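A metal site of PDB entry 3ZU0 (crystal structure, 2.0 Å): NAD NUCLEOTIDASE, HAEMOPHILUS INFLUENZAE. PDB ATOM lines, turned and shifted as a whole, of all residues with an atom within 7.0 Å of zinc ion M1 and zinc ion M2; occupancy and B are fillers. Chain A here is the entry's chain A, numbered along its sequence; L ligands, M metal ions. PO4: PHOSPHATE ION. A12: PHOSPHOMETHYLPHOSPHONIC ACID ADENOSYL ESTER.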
ATOM      1  N   ASN A  19      28.606   4.588  15.089  1.00  0.00           N
ATOM      2  CA  ASN A  19      27.356   3.832  15.226  1.00  0.00           C
ATOM      3  C   ASN A  19      26.430   4.135  14.082  1.00  0.00           C
ATOM      4  O   ASN A  19      26.475   5.219  13.516  1.00  0.00           O
ATOM      5  CB  ASN A  19      26.669   4.181  16.542  1.00  0.00           C
ATOM      6  CG  ASN A  19      26.321   5.655  16.621  1.00  0.00           C
ATOM      7  OD1 ASN A  19      27.183   6.489  16.957  1.00  0.00           O
ATOM      8  ND2 ASN A  19      25.078   6.008  16.287  1.00  0.00           N
ATOM      9  N   ASP A  20      25.565   3.185  13.750  1.00  0.00           N
ATOM     10  CA  ASP A  20      24.481   3.417  12.814  1.00  0.00           C
ATOM     11  C   ASP A  20      24.998   3.974  11.475  1.00  0.00           C
ATOM     12  O   ASP A  20      24.424   4.942  10.935  1.00  0.00           O
ATOM     13  CB  ASP A  20      23.443   4.387  13.410  1.00  0.00           C
ATOM     14  CG  ASP A  20      22.737   3.810  14.631  1.00  0.00           C
ATOM     15  OD1 ASP A  20      21.738   3.081  14.460  1.00  0.00           O
ATOM     16  OD2 ASP A  20      23.179   4.064  15.766  1.00  0.00           O
ATOM     17  N   HIS A  21      26.053   3.363  10.921  1.00  0.00           N
ATOM     18  CA  HIS A  21      26.515   3.879   9.621  1.00  0.00           C
ATOM     19  C   HIS A  21      25.542   3.463   8.528  1.00  0.00           C
ATOM     20  O   HIS A  21      25.460   4.114   7.486  1.00  0.00           O
ATOM     21  CB  HIS A  21      27.987   3.566   9.327  1.00  0.00           C
ATOM     22  CG  HIS A  21      28.243   2.204   8.761  1.00  0.00           C
ATOM     23  ND1 HIS A  21      28.604   1.124   9.548  1.00  0.00           N
ATOM     24  CD2 HIS A  21      28.277   1.763   7.483  1.00  0.00           C
ATOM     25  CE1 HIS A  21      28.813   0.072   8.778  1.00  0.00           C
ATOM     26  NE2 HIS A  21      28.616   0.433   7.519  1.00  0.00           N
ATOM     27  N   HIS A  22      24.760   2.405   8.787  1.00  0.00           N
ATOM     28  CA  HIS A  22      23.692   1.997   7.894  1.00  0.00           C
ATOM     29  C   HIS A  22      24.118   1.884   6.415  1.00  0.00           C
ATOM     30  O   HIS A  22      23.411   2.357   5.539  1.00  0.00           O
ATOM     31  CB  HIS A  22      22.514   2.971   8.005  1.00  0.00           C
ATOM     32  CG  HIS A  22      21.644   2.743   9.197  1.00  0.00           C
ATOM     33  ND1 HIS A  22      20.682   1.757   9.243  1.00  0.00           N
ATOM     34  CD2 HIS A  22      21.586   3.385  10.395  1.00  0.00           C
ATOM     35  CE1 HIS A  22      20.081   1.790  10.416  1.00  0.00           C
ATOM     36  NE2 HIS A  22      20.602   2.773  11.130  1.00  0.00           N
ATOM     37  N   ALA A  68      28.822   0.730  17.523  1.00  0.00           N
ATOM     38  CA  ALA A  68      27.688   0.480  18.401  1.00  0.00           C
ATOM     39  C   ALA A  68      26.418   0.012  17.670  1.00  0.00           C
ATOM     40  O   ALA A  68      25.329   0.137  18.210  1.00  0.00           O
ATOM     41  CB  ALA A  68      27.382   1.725  19.229  1.00  0.00           C
ATOM     42  N   GLY A  69      26.556  -0.507  16.443  1.00  0.00           N
ATOM     43  CA  GLY A  69      25.468  -1.216  15.795  1.00  0.00           C
ATOM     44  C   GLY A  69      24.729  -0.557  14.646  1.00  0.00           C
ATOM     45  O   GLY A  69      24.880   0.643  14.400  1.00  0.00           O
ATOM     46  N   ASP A  70      23.890  -1.329  13.960  1.00  0.00           N
ATOM     47  CA  ASP A  70      23.265  -0.910  12.688  1.00  0.00           C
ATOM     48  C   ASP A  70      24.358  -0.556  11.689  1.00  0.00           C
ATOM     49  O   ASP A  70      24.393   0.551  11.151  1.00  0.00           O
ATOM     50  CB  ASP A  70      22.308   0.293  12.856  1.00  0.00           C
ATOM     51  CG  ASP A  70      20.984  -0.091  13.444  1.00  0.00           C
ATOM     52  OD1 ASP A  70      20.725  -1.292  13.677  1.00  0.00           O
ATOM     53  OD2 ASP A  70      20.158   0.834  13.620  1.00  0.00           O
ATOM     54  N   GLY A 101      22.656  -4.228  16.305  1.00  0.00           N
ATOM     55  CA  GLY A 101      21.550  -3.297  16.413  1.00  0.00           C
ATOM     56  C   GLY A 101      20.231  -3.926  15.994  1.00  0.00           C
ATOM     57  O   GLY A 101      20.138  -5.126  15.836  1.00  0.00           O
ATOM     58  N   ASN A 102      19.178  -3.123  15.821  1.00  0.00           N
ATOM     59  CA  ASN A 102      17.906  -3.687  15.401  1.00  0.00           C
ATOM     60  C   ASN A 102      17.892  -4.042  13.904  1.00  0.00           C
ATOM     61  O   ASN A 102      17.370  -5.075  13.512  1.00  0.00           O
ATOM     62  CB  ASN A 102      16.731  -2.766  15.751  1.00  0.00           C
ATOM     63  CG  ASN A 102      16.952  -1.338  15.309  1.00  0.00           C
ATOM     64  OD1 ASN A 102      18.057  -0.826  15.394  1.00  0.00           O
ATOM     65  ND2 ASN A 102      15.905  -0.697  14.796  1.00  0.00           N
ATOM     66  N   HIS A 103      18.480  -3.189  13.069  1.00  0.00           N
ATOM     67  CA  HIS A 103      18.479  -3.428  11.617  1.00  0.00           C
ATOM     68  C   HIS A 103      19.376  -4.562  11.153  1.00  0.00           C
ATOM     69  O   HIS A 103      19.295  -4.998  10.027  1.00  0.00           O
ATOM     70  CB  HIS A 103      18.753  -2.139  10.833  1.00  0.00           C
ATOM     71  CG  HIS A 103      17.660  -1.134  10.985  1.00  0.00           C
ATOM     72  ND1 HIS A 103      16.522  -1.143  10.204  1.00  0.00           N
ATOM     73  CD2 HIS A 103      17.497  -0.123  11.871  1.00  0.00           C
ATOM     74  CE1 HIS A 103      15.718  -0.166  10.583  1.00  0.00           C
ATOM     75  NE2 HIS A 103      16.283   0.470  11.593  1.00  0.00           N
ATOM     76  N   GLU A 104      20.209  -5.061  12.045  1.00  0.00           N
ATOM     77  CA  GLU A 104      20.997  -6.263  11.728  1.00  0.00           C
ATOM     78  C   GLU A 104      20.112  -7.453  11.380  1.00  0.00           C
ATOM     79  O   GLU A 104      20.549  -8.360  10.653  1.00  0.00           O
ATOM     80  CB  GLU A 104      21.906  -6.626  12.919  1.00  0.00           C
ATOM     81  CG  GLU A 104      23.387  -6.279  12.718  1.00  0.00           C
ATOM     82  CD  GLU A 104      23.644  -4.795  12.735  1.00  0.00           C
ATOM     83  OE1 GLU A 104      23.295  -4.131  13.738  1.00  0.00           O
ATOM     84  OE2 GLU A 104      24.227  -4.274  11.755  1.00  0.00           O
ATOM     85  N   ASP A 159      21.351  -4.864  22.888  1.00  0.00           N
ATOM     86  CA  ASP A 159      20.550  -4.475  21.735  1.00  0.00           C
ATOM     87  C   ASP A 159      19.218  -3.951  22.229  1.00  0.00           C
ATOM     88  O   ASP A 159      18.776  -4.284  23.341  1.00  0.00           O
ATOM     89  CB  ASP A 159      20.324  -5.683  20.823  1.00  0.00           C
ATOM     90  CG  ASP A 159      19.945  -5.297  19.392  1.00  0.00           C
ATOM     91  OD1 ASP A 159      19.631  -4.117  19.114  1.00  0.00           O
ATOM     92  OD2 ASP A 159      19.954  -6.210  18.531  1.00  0.00           O
ATOM     93  N   THR A 160      18.574  -3.138  21.393  1.00  0.00           N
ATOM     94  CA  THR A 160      17.212  -2.705  21.652  1.00  0.00           C
ATOM     95  C   THR A 160      16.295  -3.884  21.359  1.00  0.00           C
ATOM     96  O   THR A 160      16.575  -4.684  20.470  1.00  0.00           O
ATOM     97  CB  THR A 160      16.827  -1.457  20.843  1.00  0.00           C
ATOM     98  OG1 THR A 160      15.564  -0.952  21.299  1.00  0.00           O
ATOM     99  CG2 THR A 160      16.756  -1.754  19.343  1.00  0.00           C
ATOM    100  N   LYS A 163      11.838  -2.810  19.221  1.00  0.00           N
ATOM    101  CA  LYS A 163      11.948  -2.421  17.811  1.00  0.00           C
ATOM    102  C   LYS A 163      12.478  -3.565  16.964  1.00  0.00           C
ATOM    103  O   LYS A 163      12.110  -3.707  15.813  1.00  0.00           O
ATOM    104  CB  LYS A 163      12.841  -1.194  17.620  1.00  0.00           C
ATOM    105  CG  LYS A 163      12.182   0.122  18.025  1.00  0.00           C
ATOM    106  CD  LYS A 163      13.194   1.268  18.092  1.00  0.00           C
ATOM    107  CE  LYS A 163      13.693   1.658  16.730  1.00  0.00           C
ATOM    108  NZ  LYS A 163      14.529   2.892  16.859  1.00  0.00           N
ATOM    109  N   HIS A 203      23.205  -0.678  21.703  1.00  0.00           N
ATOM    110  CA  HIS A 203      22.273  -0.173  20.702  1.00  0.00           C
ATOM    111  C   HIS A 203      20.860  -0.028  21.272  1.00  0.00           C
ATOM    112  O   HIS A 203      19.867  -0.059  20.554  1.00  0.00           O
ATOM    113  CB  HIS A 203      22.255  -1.093  19.475  1.00  0.00           C
ATOM    114  CG  HIS A 203      21.786  -0.427  18.226  1.00  0.00           C
ATOM    115  ND1 HIS A 203      22.631   0.301  17.416  1.00  0.00           N
ATOM    116  CD2 HIS A 203      20.562  -0.372  17.653  1.00  0.00           C
ATOM    117  CE1 HIS A 203      21.943   0.775  16.391  1.00  0.00           C
ATOM    118  NE2 HIS A 203      20.687   0.371  16.505  1.00  0.00           N
ATOM    119  N   GLY A 225      24.147   3.521  20.545  1.00  0.00           N
ATOM    120  CA  GLY A 225      23.658   3.455  19.169  1.00  0.00           C
ATOM    121  C   GLY A 225      22.136   3.456  19.135  1.00  0.00           C
ATOM    122  O   GLY A 225      21.482   3.379  20.185  1.00  0.00           O
ATOM    123  N   ASP A 226      21.570   3.553  17.923  1.00  0.00           N
ATOM    124  CA  ASP A 226      20.123   3.474  17.666  1.00  0.00           C
ATOM    125  C   ASP A 226      19.300   4.765  17.637  1.00  0.00           C
ATOM    126  O   ASP A 226      18.267   4.816  16.970  1.00  0.00           O
ATOM    127  CB  ASP A 226      19.397   2.443  18.542  1.00  0.00           C
ATOM    128  CG  ASP A 226      17.958   2.200  18.050  1.00  0.00           C
ATOM    129  OD1 ASP A 226      17.797   1.641  16.954  1.00  0.00           O
ATOM    130  OD2 ASP A 226      16.989   2.561  18.725  1.00  0.00           O
ATOM    131  N   SER A 227      19.719   5.813  18.343  1.00  0.00           N
ATOM    132  CA  SER A 227      18.913   7.022  18.299  1.00  0.00           C
ATOM    133  C   SER A 227      19.394   8.014  17.223  1.00  0.00           C
ATOM    134  O   SER A 227      18.669   8.937  16.854  1.00  0.00           O
ATOM    135  CB  SER A 227      18.802   7.672  19.690  1.00  0.00           C
ATOM    136  OG  SER A 227      20.060   7.667  20.381  1.00  0.00           O
ATOM    137  N   HIS A 228      20.593   7.809  16.713  1.00  0.00           N
ATOM    138  CA  HIS A 228      21.119   8.681  15.666  1.00  0.00           C
ATOM    139  C   HIS A 228      21.325  10.134  16.134  1.00  0.00           C
ATOM    140  O   HIS A 228      21.384  11.037  15.294  1.00  0.00           O
ATOM    141  CB  HIS A 228      20.225   8.671  14.419  1.00  0.00           C
ATOM    142  CG  HIS A 228      20.128   7.347  13.728  1.00  0.00           C
ATOM    143  ND1 HIS A 228      19.682   7.221  12.431  1.00  0.00           N
ATOM    144  CD2 HIS A 228      20.400   6.086  14.155  1.00  0.00           C
ATOM    145  CE1 HIS A 228      19.682   5.942  12.087  1.00  0.00           C
ATOM    146  NE2 HIS A 228      20.123   5.230  13.112  1.00  0.00           N
ATOM    147  N   GLU A 263      26.770   9.165  21.951  1.00  0.00           N
ATOM    148  CA  GLU A 263      26.493   8.590  20.641  1.00  0.00           C
ATOM    149  C   GLU A 263      27.321   9.373  19.625  1.00  0.00           C
ATOM    150  O   GLU A 263      27.875  10.424  19.945  1.00  0.00           O
ATOM    151  CB  GLU A 263      25.005   8.739  20.309  1.00  0.00           C
ATOM    152  CG  GLU A 263      24.535   7.945  19.078  1.00  0.00           C
ATOM    153  CD  GLU A 263      23.001   7.733  19.051  1.00  0.00           C
ATOM    154  OE1 GLU A 263      22.247   8.530  19.648  1.00  0.00           O
ATOM    155  OE2 GLU A 263      22.556   6.747  18.439  1.00  0.00           O
ATOM    156  N   ALA A 266      25.162   9.562  13.122  1.00  0.00           N
ATOM    157  CA  ALA A 266      24.863   8.408  12.273  1.00  0.00           C
ATOM    158  C   ALA A 266      25.472   8.582  10.887  1.00  0.00           C
ATOM    159  O   ALA A 266      26.089   9.612  10.610  1.00  0.00           O
ATOM    160  CB  ALA A 266      23.344   8.213  12.136  1.00  0.00           C
ATOM    161  N   TYR A 267      25.255   7.566  10.035  1.00  0.00           N
ATOM    162  CA  TYR A 267      25.604   7.596   8.601  1.00  0.00           C
ATOM    163  C   TYR A 267      27.077   7.961   8.335  1.00  0.00           C
ATOM    164  O   TYR A 267      27.383   8.732   7.420  1.00  0.00           O
ATOM    165  CB  TYR A 267      24.662   8.541   7.848  1.00  0.00           C
ATOM    166  CG  TYR A 267      23.189   8.262   8.064  1.00  0.00           C
ATOM    167  CD1 TYR A 267      22.727   6.970   8.279  1.00  0.00           C
ATOM    168  CD2 TYR A 267      22.262   9.291   8.089  1.00  0.00           C
ATOM    169  CE1 TYR A 267      21.377   6.706   8.502  1.00  0.00           C
ATOM    170  CE2 TYR A 267      20.909   9.048   8.319  1.00  0.00           C
ATOM    171  CZ  TYR A 267      20.477   7.752   8.519  1.00  0.00           C
ATOM    172  OH  TYR A 267      19.146   7.492   8.738  1.00  0.00           O
HETATM  173  P   PO4 L   1      17.068   3.137  13.908  1.00  0.00           P
HETATM  174  O1  PO4 L   1      16.629   4.292  14.798  1.00  0.00           O
HETATM  175  O2  PO4 L   1      18.396   2.621  14.450  1.00  0.00           O
HETATM  176  O3  PO4 L   1      16.018   2.050  14.063  1.00  0.00           O
HETATM  177  O4  PO4 L   1      17.223   3.575  12.469  1.00  0.00           O
HETATM  178  PB  A12 L   2      15.341   3.588   9.402  1.00  0.00           P
HETATM  179  O1B A12 L   2      15.143   4.878   8.531  1.00  0.00           O
HETATM  180  O2B A12 L   2      15.348   2.416   8.443  1.00  0.00           O
HETATM  181  O3B A12 L   2      16.619   3.628  10.132  1.00  0.00           O
HETATM  182  PA  A12 L   2      12.489   2.967   9.863  1.00  0.00           P
HETATM  183  O1A A12 L   2      12.648   3.141   8.346  1.00  0.00           O
HETATM  184  O2A A12 L   2      11.208   3.552  10.512  1.00  0.00           O
HETATM  185  C3A A12 L   2      14.024   3.393  10.465  1.00  0.00           C
HETATM  186  O5' A12 L   2      12.774   1.370  10.029  1.00  0.00           O
HETATM  187  C5' A12 L   2      11.721   0.542  10.408  1.00  0.00           C
HETATM  188  C4' A12 L   2      10.641   0.377   9.485  1.00  0.00           C
HETATM  189  O4' A12 L   2      11.160  -0.320   8.315  1.00  0.00           O
HETATM  190  C3' A12 L   2       9.659  -0.603   9.968  1.00  0.00           C
HETATM  191  O3' A12 L   2       8.754  -0.093  10.860  1.00  0.00           O
HETATM  192  C2' A12 L   2       9.006  -1.093   8.722  1.00  0.00           C
HETATM  193  O2' A12 L   2       7.976  -0.267   8.343  1.00  0.00           O
HETATM  194  C1' A12 L   2      10.116  -1.057   7.739  1.00  0.00           C
HETATM  195  N9  A12 L   2      10.567  -2.400   7.458  1.00  0.00           N
HETATM  196  C8  A12 L   2      11.578  -3.053   8.083  1.00  0.00           C
HETATM  197  N7  A12 L   2      11.654  -4.262   7.536  1.00  0.00           N
HETATM  198  C5  A12 L   2      10.695  -4.384   6.541  1.00  0.00           C
HETATM  199  C6  A12 L   2      10.321  -5.411   5.636  1.00  0.00           C
HETATM  200  N6  A12 L   2      10.950  -6.663   5.595  1.00  0.00           N
HETATM  201  N1  A12 L   2       9.338  -5.168   4.784  1.00  0.00           N
HETATM  202  C2  A12 L   2       8.691  -4.012   4.786  1.00  0.00           C
HETATM  203  N3  A12 L   2       9.004  -3.013   5.625  1.00  0.00           N
HETATM  204  C4  A12 L   2      10.000  -3.195   6.503  1.00  0.00           C
HETATM  205 ZN    ZN M   1      20.100   3.138  13.158  1.00  0.00          ZN
HETATM  206 ZN    ZN M   2      19.088   0.953  15.382  1.00  0.00          ZN
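An oxygen (O3B) of A12 L2 lies within hydrogen-bond range of a ring nitrogen (NE2) of His 103 (3.5 Å).
The backbone NH (N) of Asp 70 lies within hydrogen-bond range of the side-chain carboxylate (OE1) of Glu 104, at 2.9 Å.
The backbone carbonyl oxygen of Ala 68 lies within hydrogen-bond range of a ring nitrogen (ND1) of His 203.
The side-chain carboxylate of Asp 20 sits at hydrogen-bond distance from the backbone NH of Asp 226 (2.7 Å).
N of Asp 226 is in hydrogen-bond range of OE2 of Glu 263 (3.4 Å).
NE2 of His 103 lies close to ND2 of Asn 102, at 3.4 Å.
N of Asn 102 is in hydrogen-bond range of OD1 of Asp 159, 3.5 Å away.
The backbone carbonyl oxygen (O) of Asp 20 is in hydrogen-bond range of the backbone NH (N) of Tyr 267 (2.9 Å).
ND2 of Asn 19 sits at hydrogen-bond distance from OD2 of Asp 20, 2.8 Å away.
The nearest printed residue that does not touch zinc ion M1 is His 103 (4.4 Å).
Within 4 Å of zinc ion M2: Asp 20, Asp 70, Asn 102, His 203 and Asp 226.
Zinc ion M1 is bound by a ring nitrogen (NE2) of His 228, the side-chain carboxylate (OD1) of Asp 20, a ring nitrogen (NE2) of His 22, an oxygen (O2) of PO4 L1 and the side-chain carboxylate (OD2) of Asp 70.
Zinc ion M2 is bound by O2 of PO4 L1 (2.0 Å), NE2 of His 203 (2.0 Å), OD1 of Asn 102 (2.1 Å), OD2 of Asp 70 (2.1 Å) and OD1 of Asp 226 (2.1 Å).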
